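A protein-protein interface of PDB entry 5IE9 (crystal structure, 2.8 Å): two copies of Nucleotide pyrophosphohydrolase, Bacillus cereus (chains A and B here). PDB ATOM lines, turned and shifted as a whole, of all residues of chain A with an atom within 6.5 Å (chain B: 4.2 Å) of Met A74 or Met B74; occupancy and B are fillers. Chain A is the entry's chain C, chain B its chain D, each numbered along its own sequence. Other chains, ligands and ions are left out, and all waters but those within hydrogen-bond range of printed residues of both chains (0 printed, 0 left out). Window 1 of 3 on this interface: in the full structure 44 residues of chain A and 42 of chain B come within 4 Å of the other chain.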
ATOM      1  N   GLN A  10      34.061   2.096  13.086  1.00  0.00           N
ATOM      2  CA  GLN A  10      34.487   0.764  13.528  1.00  0.00           C
ATOM      3  C   GLN A  10      35.381   0.830  14.771  1.00  0.00           C
ATOM      4  O   GLN A  10      35.173   0.063  15.715  1.00  0.00           O
ATOM      5  CB  GLN A  10      35.145  -0.029  12.385  1.00  0.00           C
ATOM      6  CG  GLN A  10      34.163  -0.444  11.297  1.00  0.00           C
ATOM      7  CD  GLN A  10      34.739  -1.378  10.252  1.00  0.00           C
ATOM      8  OE1 GLN A  10      34.875  -1.011   9.087  1.00  0.00           O
ATOM      9  NE2 GLN A  10      35.052  -2.602  10.654  1.00  0.00           N
ATOM     10  N   LEU A  34      21.869 -10.011  14.539  1.00  0.00           N
ATOM     11  CA  LEU A  34      21.502  -9.394  13.266  1.00  0.00           C
ATOM     12  C   LEU A  34      20.096  -9.721  12.802  1.00  0.00           C
ATOM     13  O   LEU A  34      19.390  -8.832  12.307  1.00  0.00           O
ATOM     14  CB  LEU A  34      22.467  -9.800  12.165  1.00  0.00           C
ATOM     15  CG  LEU A  34      23.430  -8.723  11.719  1.00  0.00           C
ATOM     16  CD1 LEU A  34      24.509  -9.386  10.890  1.00  0.00           C
ATOM     17  CD2 LEU A  34      22.718  -7.617  10.949  1.00  0.00           C
ATOM     18  N   MET A  38      17.204  -6.922  12.269  1.00  0.00           N
ATOM     19  CA  MET A  38      16.561  -6.843  10.961  1.00  0.00           C
ATOM     20  C   MET A  38      15.041  -6.921  11.088  1.00  0.00           C
ATOM     21  O   MET A  38      14.313  -6.272  10.325  1.00  0.00           O
ATOM     22  CB  MET A  38      17.078  -7.955  10.055  1.00  0.00           C
ATOM     23  CG  MET A  38      17.109  -7.611   8.575  1.00  0.00           C
ATOM     24  SD  MET A  38      18.556  -6.614   8.173  1.00  0.00           S
ATOM     25  CE  MET A  38      17.909  -4.956   8.179  1.00  0.00           C
ATOM     26  N   LEU A  41      13.817  -3.535  12.195  1.00  0.00           N
ATOM     27  CA  LEU A  41      13.759  -2.704  11.000  1.00  0.00           C
ATOM     28  C   LEU A  41      12.533  -3.048  10.156  1.00  0.00           C
ATOM     29  O   LEU A  41      11.801  -2.140   9.755  1.00  0.00           O
ATOM     30  CB  LEU A  41      15.049  -2.785  10.167  1.00  0.00           C
ATOM     31  CG  LEU A  41      15.136  -1.929   8.893  1.00  0.00           C
ATOM     32  CD1 LEU A  41      14.908  -0.441   9.151  1.00  0.00           C
ATOM     33  CD2 LEU A  41      16.468  -2.129   8.208  1.00  0.00           C
ATOM     34  N   GLU A  66      16.504   2.442  13.738  1.00  0.00           N
ATOM     35  CA  GLU A  66      16.550   0.989  13.550  1.00  0.00           C
ATOM     36  C   GLU A  66      17.590   0.575  12.510  1.00  0.00           C
ATOM     37  O   GLU A  66      18.145  -0.516  12.611  1.00  0.00           O
ATOM     38  CB  GLU A  66      15.168   0.366  13.278  1.00  0.00           C
ATOM     39  CG  GLU A  66      14.159   0.466  14.428  1.00  0.00           C
ATOM     40  CD  GLU A  66      14.527  -0.295  15.711  1.00  0.00           C
ATOM     41  OE1 GLU A  66      15.477  -1.118  15.724  1.00  0.00           O
ATOM     42  OE2 GLU A  66      13.834  -0.076  16.733  1.00  0.00           O
ATOM     43  N   LEU A  67      17.865   1.442  11.536  1.00  0.00           N
ATOM     44  CA  LEU A  67      19.015   1.259  10.645  1.00  0.00           C
ATOM     45  C   LEU A  67      20.339   1.294  11.420  1.00  0.00           C
ATOM     46  O   LEU A  67      21.179   0.405  11.253  1.00  0.00           O
ATOM     47  CB  LEU A  67      19.022   2.295   9.517  1.00  0.00           C
ATOM     48  CG  LEU A  67      18.100   2.051   8.320  1.00  0.00           C
ATOM     49  CD1 LEU A  67      17.860   3.353   7.574  1.00  0.00           C
ATOM     50  CD2 LEU A  67      18.677   1.005   7.383  1.00  0.00           C
ATOM     51  N   ASP A  69      20.787   0.653  14.554  1.00  0.00           N
ATOM     52  CA  ASP A  69      20.792  -0.598  15.317  1.00  0.00           C
ATOM     53  C   ASP A  69      21.352  -1.773  14.510  1.00  0.00           C
ATOM     54  O   ASP A  69      22.181  -2.535  15.015  1.00  0.00           O
ATOM     55  CB  ASP A  69      19.378  -0.938  15.801  1.00  0.00           C
ATOM     56  CG  ASP A  69      19.032  -0.328  17.161  1.00  0.00           C
ATOM     57  OD1 ASP A  69      19.922   0.204  17.879  1.00  0.00           O
ATOM     58  OD2 ASP A  69      17.832  -0.406  17.516  1.00  0.00           O
ATOM     59  N   VAL A  70      20.900  -1.902  13.262  1.00  0.00           N
ATOM     60  CA  VAL A  70      21.394  -2.933  12.348  1.00  0.00           C
ATOM     61  C   VAL A  70      22.867  -2.681  12.034  1.00  0.00           C
ATOM     62  O   VAL A  70      23.682  -3.600  12.123  1.00  0.00           O
ATOM     63  CB  VAL A  70      20.550  -3.034  11.055  1.00  0.00           C
ATOM     64  CG1 VAL A  70      21.097  -4.114  10.148  1.00  0.00           C
ATOM     65  CG2 VAL A  70      19.102  -3.369  11.383  1.00  0.00           C
ATOM     66  N   LEU A  71      23.200  -1.428  11.723  1.00  0.00           N
ATOM     67  CA  LEU A  71      24.563  -1.020  11.393  1.00  0.00           C
ATOM     68  C   LEU A  71      25.550  -1.308  12.528  1.00  0.00           C
ATOM     69  O   LEU A  71      26.696  -1.677  12.274  1.00  0.00           O
ATOM     70  CB  LEU A  71      24.595   0.472  11.043  1.00  0.00           C
ATOM     71  CG  LEU A  71      25.547   1.123  10.017  1.00  0.00           C
ATOM     72  CD1 LEU A  71      26.065   2.415  10.625  1.00  0.00           C
ATOM     73  CD2 LEU A  71      26.722   0.278   9.533  1.00  0.00           C
ATOM     74  N   PHE A  72      25.101  -1.141  13.772  1.00  0.00           N
ATOM     75  CA  PHE A  72      25.945  -1.396  14.941  1.00  0.00           C
ATOM     76  C   PHE A  72      26.371  -2.861  15.011  1.00  0.00           C
ATOM     77  O   PHE A  72      27.556  -3.147  15.187  1.00  0.00           O
ATOM     78  CB  PHE A  72      25.251  -0.954  16.241  1.00  0.00           C
ATOM     79  CG  PHE A  72      26.025  -1.283  17.493  1.00  0.00           C
ATOM     80  CD1 PHE A  72      27.082  -0.480  17.909  1.00  0.00           C
ATOM     81  CD2 PHE A  72      25.690  -2.402  18.269  1.00  0.00           C
ATOM     82  CE1 PHE A  72      27.794  -0.779  19.070  1.00  0.00           C
ATOM     83  CE2 PHE A  72      26.402  -2.710  19.429  1.00  0.00           C
ATOM     84  CZ  PHE A  72      27.459  -1.897  19.828  1.00  0.00           C
ATOM     85  N   VAL A  73      25.401  -3.768  14.853  1.00  0.00           N
ATOM     86  CA  VAL A  73      25.632  -5.213  14.947  1.00  0.00           C
ATOM     87  C   VAL A  73      26.526  -5.647  13.787  1.00  0.00           C
ATOM     88  O   VAL A  73      27.405  -6.493  13.962  1.00  0.00           O
ATOM     89  CB  VAL A  73      24.306  -6.020  14.992  1.00  0.00           C
ATOM     90  CG1 VAL A  73      24.560  -7.520  15.124  1.00  0.00           C
ATOM     91  CG2 VAL A  73      23.428  -5.555  16.141  1.00  0.00           C
ATOM     92  N   MET A  74      26.316  -5.040  12.620  1.00  0.00           N
ATOM     93  CA  MET A  74      27.176  -5.259  11.465  1.00  0.00           C
ATOM     94  C   MET A  74      28.623  -4.895  11.753  1.00  0.00           C
ATOM     95  O   MET A  74      29.523  -5.677  11.441  1.00  0.00           O
ATOM     96  CB  MET A  74      26.674  -4.477  10.268  1.00  0.00           C
ATOM     97  CG  MET A  74      25.724  -5.276   9.410  1.00  0.00           C
ATOM     98  SD  MET A  74      24.992  -4.243   8.135  1.00  0.00           S
ATOM     99  CE  MET A  74      23.498  -5.193   7.894  1.00  0.00           C
ATOM    100  N   ILE A  75      28.831  -3.719  12.360  1.00  0.00           N
ATOM    101  CA  ILE A  75      30.163  -3.250  12.724  1.00  0.00           C
ATOM    102  C   ILE A  75      30.782  -4.222  13.730  1.00  0.00           C
ATOM    103  O   ILE A  75      31.933  -4.625  13.571  1.00  0.00           O
ATOM    104  CB  ILE A  75      30.163  -1.782  13.220  1.00  0.00           C
ATOM    105  CG1 ILE A  75      29.908  -0.830  12.041  1.00  0.00           C
ATOM    106  CG2 ILE A  75      31.499  -1.432  13.862  1.00  0.00           C
ATOM    107  CD1 ILE A  75      29.522   0.589  12.418  1.00  0.00           C
ATOM    108  N   CYS A  76      29.994  -4.621  14.727  1.00  0.00           N
ATOM    109  CA  CYS A  76      30.392  -5.657  15.682  1.00  0.00           C
ATOM    110  C   CYS A  76      30.848  -6.940  14.984  1.00  0.00           C
ATOM    111  O   CYS A  76      31.945  -7.431  15.256  1.00  0.00           O
ATOM    112  CB  CYS A  76      29.261  -5.955  16.662  1.00  0.00           C
ATOM    113  SG  CYS A  76      29.001  -4.642  17.862  1.00  0.00           S
ATOM    114  N   MET A  77      30.014  -7.448  14.074  1.00  0.00           N
ATOM    115  CA  MET A  77      30.318  -8.621  13.263  1.00  0.00           C
ATOM    116  C   MET A  77      31.665  -8.437  12.549  1.00  0.00           C
ATOM    117  O   MET A  77      32.553  -9.292  12.654  1.00  0.00           O
ATOM    118  CB  MET A  77      29.168  -8.864  12.273  1.00  0.00           C
ATOM    119  CG  MET A  77      29.381  -9.958  11.233  1.00  0.00           C
ATOM    120  SD  MET A  77      29.073 -11.610  11.876  1.00  0.00           S
ATOM    121  CE  MET A  77      27.296 -11.749  11.671  1.00  0.00           C
ATOM    122  N   ALA A  78      31.815  -7.300  11.868  1.00  0.00           N
ATOM    123  CA  ALA A  78      33.000  -7.004  11.075  1.00  0.00           C
ATOM    124  C   ALA A  78      34.263  -6.883  11.932  1.00  0.00           C
ATOM    125  O   ALA A  78      35.325  -7.376  11.546  1.00  0.00           O
ATOM    126  CB  ALA A  78      32.781  -5.747  10.249  1.00  0.00           C
ATOM    127  N   ASN A  79      34.134  -6.238  13.092  1.00  0.00           N
ATOM    128  CA  ASN A  79      35.242  -6.073  14.026  1.00  0.00           C
ATOM    129  C   ASN A  79      35.677  -7.403  14.615  1.00  0.00           C
ATOM    130  O   ASN A  79      36.867  -7.713  14.638  1.00  0.00           O
ATOM    131  CB  ASN A  79      34.858  -5.123  15.152  1.00  0.00           C
ATOM    132  CG  ASN A  79      34.715  -3.673  14.708  1.00  0.00           C
ATOM    133  OD1 ASN A  79      34.365  -2.821  15.523  1.00  0.00           O
ATOM    134  ND2 ASN A  79      34.979  -3.381  13.437  1.00  0.00           N
ATOM    135  N   LEU A  85      35.015  -2.714   6.750  1.00  0.00           N
ATOM    136  CA  LEU A  85      33.813  -2.485   5.919  1.00  0.00           C
ATOM    137  C   LEU A  85      34.002  -1.504   4.747  1.00  0.00           C
ATOM    138  O   LEU A  85      33.185  -1.488   3.822  1.00  0.00           O
ATOM    139  CB  LEU A  85      32.606  -2.066   6.772  1.00  0.00           C
ATOM    140  CG  LEU A  85      31.975  -3.071   7.738  1.00  0.00           C
ATOM    141  CD1 LEU A  85      31.056  -2.338   8.697  1.00  0.00           C
ATOM    142  CD2 LEU A  85      31.221  -4.197   7.040  1.00  0.00           C
ATOM    143  N   LEU B  34      16.920  -6.913   1.525  1.00  0.00           N
ATOM    144  CA  LEU B  34      17.705  -6.966   2.740  1.00  0.00           C
ATOM    145  C   LEU B  34      17.612  -8.321   3.436  1.00  0.00           C
ATOM    146  O   LEU B  34      18.626  -8.828   3.930  1.00  0.00           O
ATOM    147  CB  LEU B  34      17.235  -5.866   3.671  1.00  0.00           C
ATOM    148  CG  LEU B  34      18.164  -5.206   4.674  1.00  0.00           C
ATOM    149  CD1 LEU B  34      19.647  -5.455   4.445  1.00  0.00           C
ATOM    150  CD2 LEU B  34      17.840  -3.728   4.586  1.00  0.00           C
ATOM    151  N   VAL B  70      25.297  -6.863   2.093  1.00  0.00           N
ATOM    152  CA  VAL B  70      24.259  -6.408   3.002  1.00  0.00           C
ATOM    153  C   VAL B  70      24.389  -4.896   3.222  1.00  0.00           C
ATOM    154  O   VAL B  70      23.386  -4.188   3.214  1.00  0.00           O
ATOM    155  CB  VAL B  70      24.181  -7.262   4.302  1.00  0.00           C
ATOM    156  CG1 VAL B  70      25.285  -6.926   5.287  1.00  0.00           C
ATOM    157  CG2 VAL B  70      22.840  -7.087   4.977  1.00  0.00           C
ATOM    158  N   LEU B  71      25.627  -4.410   3.332  1.00  0.00           N
ATOM    159  CA  LEU B  71      25.912  -2.985   3.509  1.00  0.00           C
ATOM    160  C   LEU B  71      25.402  -2.148   2.334  1.00  0.00           C
ATOM    161  O   LEU B  71      24.873  -1.053   2.536  1.00  0.00           O
ATOM    162  CB  LEU B  71      27.417  -2.751   3.697  1.00  0.00           C
ATOM    163  CG  LEU B  71      28.007  -1.657   4.615  1.00  0.00           C
ATOM    164  CD1 LEU B  71      29.192  -1.024   3.908  1.00  0.00           C
ATOM    165  CD2 LEU B  71      27.051  -0.560   5.078  1.00  0.00           C
ATOM    166  N   PHE B  72      25.568  -2.664   1.117  1.00  0.00           N
ATOM    167  CA  PHE B  72      25.091  -1.984  -0.088  1.00  0.00           C
ATOM    168  C   PHE B  72      23.580  -1.742  -0.043  1.00  0.00           C
ATOM    169  O   PHE B  72      23.130  -0.640  -0.354  1.00  0.00           O
ATOM    170  CB  PHE B  72      25.498  -2.747  -1.358  1.00  0.00           C
ATOM    171  CG  PHE B  72      24.903  -2.193  -2.622  1.00  0.00           C
ATOM    172  CD1 PHE B  72      25.444  -1.067  -3.230  1.00  0.00           C
ATOM    173  CD2 PHE B  72      23.794  -2.807  -3.216  1.00  0.00           C
ATOM    174  CE1 PHE B  72      24.895  -0.557  -4.405  1.00  0.00           C
ATOM    175  CE2 PHE B  72      23.237  -2.300  -4.389  1.00  0.00           C
ATOM    176  CZ  PHE B  72      23.791  -1.171  -4.985  1.00  0.00           C
ATOM    177  N   VAL B  73      22.821  -2.767   0.359  1.00  0.00           N
ATOM    178  CA  VAL B  73      21.358  -2.691   0.435  1.00  0.00           C
ATOM    179  C   VAL B  73      20.950  -1.726   1.549  1.00  0.00           C
ATOM    180  O   VAL B  73      19.999  -0.961   1.390  1.00  0.00           O
ATOM    181  CB  VAL B  73      20.703  -4.093   0.598  1.00  0.00           C
ATOM    182  CG1 VAL B  73      19.180  -4.008   0.611  1.00  0.00           C
ATOM    183  CG2 VAL B  73      21.142  -5.023  -0.521  1.00  0.00           C
ATOM    184  N   MET B  74      21.693  -1.752   2.654  1.00  0.00           N
ATOM    185  CA  MET B  74      21.541  -0.792   3.754  1.00  0.00           C
ATOM    186  C   MET B  74      21.654   0.643   3.259  1.00  0.00           C
ATOM    187  O   MET B  74      20.798   1.478   3.575  1.00  0.00           O
ATOM    188  CB  MET B  74      22.631  -1.010   4.792  1.00  0.00           C
ATOM    189  CG  MET B  74      22.580  -2.335   5.514  1.00  0.00           C
ATOM    190  SD  MET B  74      21.983  -2.069   7.168  1.00  0.00           S
ATOM    191  CE  MET B  74      20.215  -2.220   6.916  1.00  0.00           C
ATOM    192  N   ILE B  75      22.710   0.914   2.480  1.00  0.00           N
ATOM    193  CA  ILE B  75      22.978   2.246   1.954  1.00  0.00           C
ATOM    194  C   ILE B  75      21.864   2.648   0.988  1.00  0.00           C
ATOM    195  O   ILE B  75      21.372   3.779   1.045  1.00  0.00           O
ATOM    196  CB  ILE B  75      24.389   2.363   1.325  1.00  0.00           C
ATOM    197  CG1 ILE B  75      25.462   2.261   2.418  1.00  0.00           C
ATOM    198  CG2 ILE B  75      24.549   3.694   0.596  1.00  0.00           C
ATOM    199  CD1 ILE B  75      26.867   1.977   1.924  1.00  0.00           C
ATOM    200  N   CYS B  76      21.453   1.707   0.141  1.00  0.00           N
ATOM    201  CA  CYS B  76      20.315   1.897  -0.764  1.00  0.00           C
ATOM    202  C   CYS B  76      19.060   2.291   0.003  1.00  0.00           C
ATOM    203  O   CYS B  76      18.408   3.274  -0.344  1.00  0.00           O
ATOM    204  CB  CYS B  76      20.057   0.639  -1.594  1.00  0.00           C
ATOM    205  SG  CYS B  76      21.234   0.392  -2.941  1.00  0.00           S
ATOM    206  N   MET B  77      18.758   1.530   1.059  1.00  0.00           N
ATOM    207  CA  MET B  77      17.628   1.782   1.940  1.00  0.00           C
ATOM    208  C   MET B  77      17.695   3.197   2.522  1.00  0.00           C
ATOM    209  O   MET B  77      16.711   3.943   2.459  1.00  0.00           O
ATOM    210  CB  MET B  77      17.603   0.725   3.048  1.00  0.00           C
ATOM    211  CG  MET B  77      16.595   0.968   4.163  1.00  0.00           C
ATOM    212  SD  MET B  77      14.962   0.343   3.753  1.00  0.00           S
ATOM    213  CE  MET B  77      15.065  -1.306   4.446  1.00  0.00           C
ATOM    214  N   ALA B  78      18.862   3.558   3.057  1.00  0.00           N
ATOM    215  CA  ALA B  78      19.067   4.849   3.703  1.00  0.00           C
ATOM    216  C   ALA B  78      18.931   6.009   2.716  1.00  0.00           C
ATOM    217  O   ALA B  78      18.250   6.995   3.009  1.00  0.00           O
ATOM    218  CB  ALA B  78      20.414   4.887   4.407  1.00  0.00           C
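Among the printed residues, merely in contact across the chains: Met A38 with Leu B34 (3.5 Å), Met A38 with Met B74 (3.8 Å), Leu A41 with Met B74 (3.96 Å), Leu A67 with Met B74 (3.6 Å), Leu A67 with Met B77 (3.8 Å), Val A70 with Met B74 (3.7 Å), Met A74 with Val B70 (3.5 Å) and Met A74 with Met B74 (3.5 Å).
Printed residues of chain B within 4 Å of Met A38: Leu B34 (3.5 Å) and Met B74 (3.8 Å). Printed residues of chain A within 4 Å of Leu B34: Met A38 (3.5 Å). Of chain A, only Met A38, Leu A41, Leu A67, Val A70 and Met A74 come within 4 Å of Met B74. The nearest residue of chain A that does not touch Met B74 is Leu A71 (4.8 Å). The nearest printed residue of chain B that does not touch Val A70 is Leu B34 (6.0 Å).
Of the 18 printed residues of chain A, 5 touch a printed residue of chain B. Among the printed residues, 8 pairs touch across the chains. Among the printed residues, no Asp or Glu carboxylate lies within 4 Å of a Lys or Arg side-chain nitrogen of the other chain.
Val A70 touches Met B74, and with the chains exchanged Met A74 touches Val B70. Met B74 touches its own counterpart, Met A74. Positions printed for both chains: 34, 70, 71, 72, 73, 74, 75, 76, 77 and 78. Of the 8 pairs that touch across the chains among the printed residues, 3 have their exchanged pair printed and touching as well.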
